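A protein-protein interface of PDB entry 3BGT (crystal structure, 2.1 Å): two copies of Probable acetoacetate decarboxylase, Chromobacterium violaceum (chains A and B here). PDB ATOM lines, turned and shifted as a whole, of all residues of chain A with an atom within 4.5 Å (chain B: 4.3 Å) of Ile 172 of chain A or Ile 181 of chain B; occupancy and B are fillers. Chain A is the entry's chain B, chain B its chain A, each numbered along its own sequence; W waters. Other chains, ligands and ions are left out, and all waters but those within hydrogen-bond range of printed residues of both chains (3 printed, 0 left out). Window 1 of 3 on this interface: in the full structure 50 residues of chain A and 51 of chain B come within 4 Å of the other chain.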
ATOM      1  N   ARG A 109     -24.208  20.911  29.652  1.00  0.00           N
ATOM      2  CA  ARG A 109     -22.960  20.160  29.872  1.00  0.00           C
ATOM      3  C   ARG A 109     -22.006  20.225  28.668  1.00  0.00           C
ATOM      4  O   ARG A 109     -20.818  20.465  28.836  1.00  0.00           O
ATOM      5  CB  ARG A 109     -23.234  18.692  30.198  1.00  0.00           C
ATOM      6  CG  ARG A 109     -24.018  18.429  31.490  1.00  0.00           C
ATOM      7  CD  ARG A 109     -24.173  16.932  31.810  1.00  0.00           C
ATOM      8  NE  ARG A 109     -22.907  16.169  31.888  1.00  0.00           N
ATOM      9  CZ  ARG A 109     -22.125  16.069  32.966  1.00  0.00           C
ATOM     10  NH1 ARG A 109     -22.432  16.693  34.100  1.00  0.00           N
ATOM     11  NH2 ARG A 109     -20.989  15.360  32.896  1.00  0.00           N
ATOM     12  N   LYS A 170     -15.287  23.095  32.607  1.00  0.00           N
ATOM     13  CA  LYS A 170     -15.723  22.128  31.610  1.00  0.00           C
ATOM     14  C   LYS A 170     -14.765  20.935  31.533  1.00  0.00           C
ATOM     15  O   LYS A 170     -13.561  21.106  31.372  1.00  0.00           O
ATOM     16  CB  LYS A 170     -15.923  22.773  30.229  1.00  0.00           C
ATOM     17  CG  LYS A 170     -16.535  21.798  29.158  1.00  0.00           C
ATOM     18  CD  LYS A 170     -16.707  22.549  27.838  1.00  0.00           C
ATOM     19  CE  LYS A 170     -17.193  21.634  26.718  1.00  0.00           C
ATOM     20  NZ  LYS A 170     -17.609  22.548  25.574  1.00  0.00           N
ATOM     21  N   ILE A 171     -15.324  19.733  31.683  1.00  0.00           N
ATOM     22  CA  ILE A 171     -14.581  18.488  31.610  1.00  0.00           C
ATOM     23  C   ILE A 171     -15.346  17.549  30.692  1.00  0.00           C
ATOM     24  O   ILE A 171     -16.511  17.191  30.978  1.00  0.00           O
ATOM     25  CB  ILE A 171     -14.453  17.798  32.988  1.00  0.00           C
ATOM     26  CG1 ILE A 171     -13.860  18.757  34.055  1.00  0.00           C
ATOM     27  CG2 ILE A 171     -13.683  16.494  32.845  1.00  0.00           C
ATOM     28  CD1 ILE A 171     -13.615  18.117  35.425  1.00  0.00           C
ATOM     29  N   ILE A 172     -14.709  17.142  29.605  1.00  0.00           N
ATOM     30  CA  ILE A 172     -15.231  16.039  28.786  1.00  0.00           C
ATOM     31  C   ILE A 172     -14.145  14.945  28.701  1.00  0.00           C
ATOM     32  O   ILE A 172     -12.973  15.258  28.446  1.00  0.00           O
ATOM     33  CB  ILE A 172     -15.707  16.522  27.363  1.00  0.00           C
ATOM     34  CG1 ILE A 172     -16.858  17.579  27.444  1.00  0.00           C
ATOM     35  CG2 ILE A 172     -16.015  15.334  26.391  1.00  0.00           C
ATOM     36  CD1 ILE A 172     -18.248  17.109  27.916  1.00  0.00           C
ATOM     37  N   PRO A 173     -14.512  13.674  28.952  1.00  0.00           N
ATOM     38  CA  PRO A 173     -13.573  12.567  28.749  1.00  0.00           C
ATOM     39  C   PRO A 173     -13.335  12.208  27.286  1.00  0.00           C
ATOM     40  O   PRO A 173     -14.231  12.337  26.430  1.00  0.00           O
ATOM     41  CB  PRO A 173     -14.243  11.394  29.461  1.00  0.00           C
ATOM     42  CG  PRO A 173     -15.730  11.692  29.336  1.00  0.00           C
ATOM     43  CD  PRO A 173     -15.808  13.201  29.486  1.00  0.00           C
ATOM     44  N   HIS A 174     -12.100  11.777  27.025  1.00  0.00           N
ATOM     45  CA  HIS A 174     -11.732  11.152  25.768  1.00  0.00           C
ATOM     46  C   HIS A 174     -12.299   9.758  25.842  1.00  0.00           C
ATOM     47  O   HIS A 174     -12.671   9.314  26.929  1.00  0.00           O
ATOM     48  CB  HIS A 174     -10.200  11.135  25.636  1.00  0.00           C
ATOM     49  CG  HIS A 174      -9.710  10.696  24.296  1.00  0.00           C
ATOM     50  ND1 HIS A 174     -10.275  11.120  23.110  1.00  0.00           N
ATOM     51  CD2 HIS A 174      -8.688   9.875  23.953  1.00  0.00           C
ATOM     52  CE1 HIS A 174      -9.630  10.566  22.099  1.00  0.00           C
ATOM     53  NE2 HIS A 174      -8.660   9.814  22.587  1.00  0.00           N
ATOM     54  N   PRO A 179      -9.004  13.065  30.401  1.00  0.00           N
ATOM     55  CA  PRO A 179      -9.743  14.253  29.940  1.00  0.00           C
ATOM     56  C   PRO A 179      -9.356  14.760  28.549  1.00  0.00           C
ATOM     57  O   PRO A 179      -8.158  14.978  28.269  1.00  0.00           O
ATOM     58  CB  PRO A 179      -9.450  15.328  31.020  1.00  0.00           C
ATOM     59  CG  PRO A 179      -8.199  14.845  31.726  1.00  0.00           C
ATOM     60  CD  PRO A 179      -8.231  13.322  31.638  1.00  0.00           C
ATOM     61  N   ARG A 180     -10.361  14.957  27.700  1.00  0.00           N
ATOM     62  CA  ARG A 180     -10.154  15.450  26.344  1.00  0.00           C
ATOM     63  C   ARG A 180     -10.328  16.968  26.331  1.00  0.00           C
ATOM     64  O   ARG A 180      -9.621  17.682  25.616  1.00  0.00           O
ATOM     65  CB  ARG A 180     -11.102  14.743  25.358  1.00  0.00           C
ATOM     66  CG  ARG A 180     -11.113  15.256  23.898  1.00  0.00           C
ATOM     67  CD  ARG A 180      -9.829  14.907  23.119  1.00  0.00           C
ATOM     68  NE  ARG A 180      -9.907  15.361  21.720  1.00  0.00           N
ATOM     69  CZ  ARG A 180     -10.477  14.679  20.726  1.00  0.00           C
ATOM     70  NH1 ARG A 180     -11.050  13.502  20.945  1.00  0.00           N
ATOM     71  NH2 ARG A 180     -10.487  15.175  19.500  1.00  0.00           N
ATOM     72  N   ILE A 181     -11.261  17.448  27.143  1.00  0.00           N
ATOM     73  CA  ILE A 181     -11.474  18.877  27.398  1.00  0.00           C
ATOM     74  C   ILE A 181     -11.407  19.040  28.909  1.00  0.00           C
ATOM     75  O   ILE A 181     -12.019  18.261  29.638  1.00  0.00           O
ATOM     76  CB  ILE A 181     -12.895  19.350  26.935  1.00  0.00           C
ATOM     77  CG1 ILE A 181     -13.115  19.134  25.433  1.00  0.00           C
ATOM     78  CG2 ILE A 181     -13.179  20.813  27.292  1.00  0.00           C
ATOM     79  CD1 ILE A 181     -14.600  19.227  25.021  1.00  0.00           C
ATOM     80  N   MET B  13     -17.806  15.903  34.582  1.00  0.00           N
ATOM     81  CA  MET B  13     -18.446  16.937  35.382  1.00  0.00           C
ATOM     82  C   MET B  13     -19.546  16.345  36.274  1.00  0.00           C
ATOM     83  O   MET B  13     -20.211  15.367  35.883  1.00  0.00           O
ATOM     84  CB  MET B  13     -19.057  18.011  34.480  1.00  0.00           C
ATOM     85  CG  MET B  13     -18.046  18.769  33.636  1.00  0.00           C
ATOM     86  SD  MET B  13     -18.944  19.925  32.413  1.00  0.00           S
ATOM     87  CE  MET B  13     -19.643  18.596  31.202  1.00  0.00           C
ATOM     88  N   GLU B 110     -20.835  11.410  26.536  1.00  0.00           N
ATOM     89  CA  GLU B 110     -19.581  12.130  26.758  1.00  0.00           C
ATOM     90  C   GLU B 110     -18.318  11.259  26.647  1.00  0.00           C
ATOM     91  O   GLU B 110     -17.236  11.770  26.277  1.00  0.00           O
ATOM     92  CB  GLU B 110     -19.598  12.919  28.065  1.00  0.00           C
ATOM     93  CG  GLU B 110     -20.749  13.922  28.075  1.00  0.00           C
ATOM     94  CD  GLU B 110     -21.049  14.538  29.429  1.00  0.00           C
ATOM     95  OE1 GLU B 110     -20.233  14.458  30.380  1.00  0.00           O
ATOM     96  OE2 GLU B 110     -22.136  15.126  29.525  1.00  0.00           O
ATOM     97  N   LYS B 170     -18.855  10.398  17.433  1.00  0.00           N
ATOM     98  CA  LYS B 170     -18.784  11.236  18.625  1.00  0.00           C
ATOM     99  C   LYS B 170     -18.581  12.726  18.284  1.00  0.00           C
ATOM    100  O   LYS B 170     -17.587  13.117  17.697  1.00  0.00           O
ATOM    101  CB  LYS B 170     -17.710  10.708  19.595  1.00  0.00           C
ATOM    102  CG  LYS B 170     -17.619  11.506  20.889  1.00  0.00           C
ATOM    103  CD  LYS B 170     -16.599  10.908  21.874  1.00  0.00           C
ATOM    104  CE  LYS B 170     -16.488  11.820  23.096  1.00  0.00           C
ATOM    105  NZ  LYS B 170     -15.573  11.312  24.117  1.00  0.00           N
ATOM    106  N   ILE B 171     -19.549  13.565  18.645  1.00  0.00           N
ATOM    107  CA  ILE B 171     -19.464  14.986  18.368  1.00  0.00           C
ATOM    108  C   ILE B 171     -19.688  15.695  19.675  1.00  0.00           C
ATOM    109  O   ILE B 171     -20.678  15.412  20.380  1.00  0.00           O
ATOM    110  CB  ILE B 171     -20.567  15.443  17.421  1.00  0.00           C
ATOM    111  CG1 ILE B 171     -20.517  14.696  16.067  1.00  0.00           C
ATOM    112  CG2 ILE B 171     -20.532  16.943  17.259  1.00  0.00           C
ATOM    113  CD1 ILE B 171     -21.825  14.822  15.330  1.00  0.00           C
ATOM    114  N   ILE B 172     -18.781  16.607  20.010  1.00  0.00           N
ATOM    115  CA  ILE B 172     -18.947  17.454  21.174  1.00  0.00           C
ATOM    116  C   ILE B 172     -18.554  18.864  20.736  1.00  0.00           C
ATOM    117  O   ILE B 172     -17.458  19.065  20.223  1.00  0.00           O
ATOM    118  CB  ILE B 172     -18.065  16.978  22.386  1.00  0.00           C
ATOM    119  CG1 ILE B 172     -18.443  15.553  22.851  1.00  0.00           C
ATOM    120  CG2 ILE B 172     -18.128  17.976  23.527  1.00  0.00           C
ATOM    121  CD1 ILE B 172     -19.695  15.451  23.762  1.00  0.00           C
ATOM    122  N   PRO B 179     -17.217  22.258  16.303  1.00  0.00           N
ATOM    123  CA  PRO B 179     -16.893  20.969  16.945  1.00  0.00           C
ATOM    124  C   PRO B 179     -15.524  20.998  17.606  1.00  0.00           C
ATOM    125  O   PRO B 179     -14.589  21.538  17.027  1.00  0.00           O
ATOM    126  CB  PRO B 179     -16.895  19.967  15.782  1.00  0.00           C
ATOM    127  CG  PRO B 179     -17.508  20.685  14.631  1.00  0.00           C
ATOM    128  CD  PRO B 179     -17.294  22.143  14.836  1.00  0.00           C
ATOM    129  N   ARG B 180     -15.422  20.445  18.813  1.00  0.00           N
ATOM    130  CA  ARG B 180     -14.135  20.271  19.491  1.00  0.00           C
ATOM    131  C   ARG B 180     -13.742  18.797  19.394  1.00  0.00           C
ATOM    132  O   ARG B 180     -12.561  18.463  19.351  1.00  0.00           O
ATOM    133  CB  ARG B 180     -14.214  20.748  20.969  1.00  0.00           C
ATOM    134  CG  ARG B 180     -13.006  20.449  21.863  1.00  0.00           C
ATOM    135  CD  ARG B 180     -11.862  21.475  21.735  1.00  0.00           C
ATOM    136  NE  ARG B 180     -10.721  21.173  22.619  1.00  0.00           N
ATOM    137  CZ  ARG B 180     -10.541  21.629  23.863  1.00  0.00           C
ATOM    138  NH1 ARG B 180     -11.430  22.425  24.448  1.00  0.00           N
ATOM    139  NH2 ARG B 180      -9.457  21.272  24.542  1.00  0.00           N
ATOM    140  N   ILE B 181     -14.753  17.927  19.359  1.00  0.00           N
ATOM    141  CA  ILE B 181     -14.572  16.502  19.131  1.00  0.00           C
ATOM    142  C   ILE B 181     -15.502  16.087  17.987  1.00  0.00           C
ATOM    143  O   ILE B 181     -16.706  16.340  18.041  1.00  0.00           O
ATOM    144  CB  ILE B 181     -14.841  15.641  20.410  1.00  0.00           C
ATOM    145  CG1 ILE B 181     -13.947  16.100  21.572  1.00  0.00           C
ATOM    146  CG2 ILE B 181     -14.564  14.194  20.130  1.00  0.00           C
ATOM    147  CD1 ILE B 181     -14.388  15.599  22.956  1.00  0.00           C
ATOM    148  N   CYS B 182     -14.941  15.475  16.943  1.00  0.00           N
ATOM    149  CA  CYS B 182     -15.739  14.922  15.839  1.00  0.00           C
ATOM    150  C   CYS B 182     -15.016  13.731  15.229  1.00  0.00           C
ATOM    151  O   CYS B 182     -14.107  13.903  14.400  1.00  0.00           O
ATOM    152  CB  CYS B 182     -16.018  15.982  14.759  1.00  0.00           C
ATOM    153  SG  CYS B 182     -17.303  15.543  13.534  1.00  0.00           S
ATOM    154  N   GLU B 183     -15.410  12.528  15.649  1.00  0.00           N
ATOM    155  CA  GLU B 183     -14.645  11.318  15.351  1.00  0.00           C
ATOM    156  C   GLU B 183     -15.498  10.050  15.301  1.00  0.00           C
ATOM    157  O   GLU B 183     -16.514   9.926  16.014  1.00  0.00           O
ATOM    158  CB  GLU B 183     -13.492  11.137  16.363  1.00  0.00           C
ATOM    159  CG  GLU B 183     -13.943  10.981  17.837  1.00  0.00           C
ATOM    160  CD  GLU B 183     -12.908  11.429  18.860  1.00  0.00           C
ATOM    161  OE1 GLU B 183     -11.957  12.172  18.521  1.00  0.00           O
ATOM    162  OE2 GLU B 183     -13.055  11.066  20.036  1.00  0.00           O
ATOM    163  N   LEU B 244     -11.455  15.672  12.405  1.00  0.00           N
ATOM    164  CA  LEU B 244     -10.836  16.934  12.702  1.00  0.00           C
ATOM    165  C   LEU B 244      -9.332  16.863  12.434  1.00  0.00           C
ATOM    166  O   LEU B 244      -8.629  17.839  12.628  1.00  0.00           O
ATOM    167  CB  LEU B 244     -11.121  17.356  14.152  1.00  0.00           C
ATOM    168  CG  LEU B 244     -12.378  18.197  14.478  1.00  0.00           C
ATOM    169  CD1 LEU B 244     -13.518  18.129  13.451  1.00  0.00           C
ATOM    170  CD2 LEU B 244     -12.902  17.914  15.864  1.00  0.00           C
HETATM  171  O   HOH W   1     -18.161  15.335  31.705  1.00  0.00           O
HETATM  172  O   HOH W   2     -13.129  11.946  22.587  1.00  0.00           O
HETATM  173  O   HOH W   3     -12.418  14.709  16.960  1.00  0.00           O
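The guanidinium group (NH2) of Arg 109 of chain A is in hydrogen-bond range of the backbone carbonyl oxygen (O) of Met 13 of chain B (3.1 Å). The backbone NH of Ile 171 of chain A sits close to the side-chain sulfur of Met 13 of chain B (3.7 Å). OE2 of Glu 110 of chain B lies within salt-bridge range of NE of Arg 109 of chain A, at 2.7 Å. The side-chain amino group (NZ) of Lys 170 of chain B sits at hydrogen-bond distance from the backbone carbonyl oxygen (O) of Pro 173 of chain A, 2.9 Å away. OE1 of Glu 183 of chain B is in salt-bridge range of NH1 of Arg 180 of chain A. The backbone carbonyl oxygen (O) of Pro 173 of chain A sits close to the backbone carbonyl oxygen (O) of Glu 110 of chain B (3.1 Å).
The side-chain amino group of Lys 170 of chain B sits at hydrogen-bond distance from the backbone carbonyl oxygen of Glu 110 of chain B, 2.8 Å away. N of Lys 170 of chain B lies within hydrogen-bond range of O of Glu 183 of chain B (2.8 Å). N of Ile 172 of chain B is in hydrogen-bond range of O of Ile 181 of chain B, at 2.9 Å. O of Ile 172 of chain A lies within hydrogen-bond range of N of Arg 180 of chain A (2.7 Å). The backbone NH of Ile 172 of chain A lies within hydrogen-bond range of the backbone carbonyl oxygen of Ile 181 of chain A, at 2.9 Å. ND1 of His 174 of chain A sits at hydrogen-bond distance from NH1 of Arg 180 of chain A (3.3 Å).
Among the printed residues, merely in contact across the chains: Lys 170 of chain A with Met 13 of chain B (3.98 Å), Ile 172 of chain A with Met 13 of chain B (3.9 Å), Ile 172 of chain A with Glu 110 of chain B (3.8 Å), Ile 172 of chain A with Ile 181 of chain B (3.8 Å), Arg 180 of chain A with Arg 180 of chain B (3.8 Å), Arg 180 of chain A with Ile 181 of chain B (3.4 Å) and Ile 181 of chain A with Arg 180 of chain B (3.7 Å).
Of the printed residues of chain B, Arg 109 of chain A touches Met 13 (3.1 Å) and Glu 110 (2.7 Å). Printed residues of chain B within 4 Å of Lys 170 of chain A: Met 13 (3.98 Å). Ile 172 of chain A touches just these residues of chain B: Met 13 (3.9 Å), Glu 110 (3.8 Å) and Ile 181 (3.8 Å). Printed residues of chain B within 4 Å of Pro 173 of chain A: Glu 110 (3.1 Å) and Lys 170 (2.9 Å). Pro 179 of chain A touches none of the printed residues of chain B. Printed residues of chain B within 4 Å of Arg 180 of chain A: Arg 180 (3.8 Å), Ile 181 (3.4 Å) and Glu 183 (2.9 Å). Printed residues of chain A within 4 Å of Met 13 of chain B: Arg 109 (3.1 Å), Lys 170 (3.98 Å), Ile 171 (3.4 Å) and Ile 172 (3.9 Å). Ile 181 of chain B touches just these residues of chain A: Ile 172 and Arg 180. The nearest residue of chain B that does not touch Ile 172 of chain A is Ile 172 of chain B (4.1 Å). The nearest printed residue of chain B that does not touch Arg 109 of chain A is Ile 172 of chain B (6.5 Å).
Printed residues of chain B that touch a printed residue of chain A: Met 13, Glu 110, Lys 170, Arg 180, Ile 181 and Glu 183. Printed residues of chain A that touch a printed residue of chain B: Arg 109, Lys 170, Ile 171, Ile 172, Pro 173, Arg 180 and Ile 181. Hydrophobic or aromatic side chains of chain A that line the printed part of chain B: Ile 171, Ile 172, Pro 173 and Ile 181. Among the printed residues, Asp or Glu carboxylates within 4 Å of a Lys or Arg side-chain nitrogen of the other chain: Arg 109 of chain A with Glu 110 of chain B (2.7 Å) and Arg 180 of chain A with Glu 183 of chain B (2.9 Å).
Ile 172 of chain A touches Ile 181 of chain B, but with the chains exchanged Ile 181 of chain A does not touch Ile 172 of chain B (4.03 Å). Arg 180 of chain A touches its own counterpart, Arg 180 of chain B. Arg 180 of chain A touches Ile 181 of chain B, and with the chains exchanged Ile 181 of chain A touches Arg 180 of chain B. Of the 13 pairs that touch across the chains among the printed residues, 3 have their exchanged pair printed and touching as well.
Water W1 lies within hydrogen-bond range of O of Ile 171 of chain A, OE1 of Glu 110 of chain B, N of Met 13 of chain B and NH2 of Arg 109 of chain A. Water W3 lies within hydrogen-bond range of N of Cys 182 of chain B (2.6 Å), OE1 of Glu 183 of chain B (3.0 Å) and NH2 of Arg 180 of chain A (3.2 Å). Water W2 lies within hydrogen-bond range of the side-chain carboxylate of Glu 183 of chain B, the side-chain amino group of Lys 170 of chain B, a ring nitrogen (ND1) of His 174 of chain A and the guanidinium group of Arg 180 of chain A.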
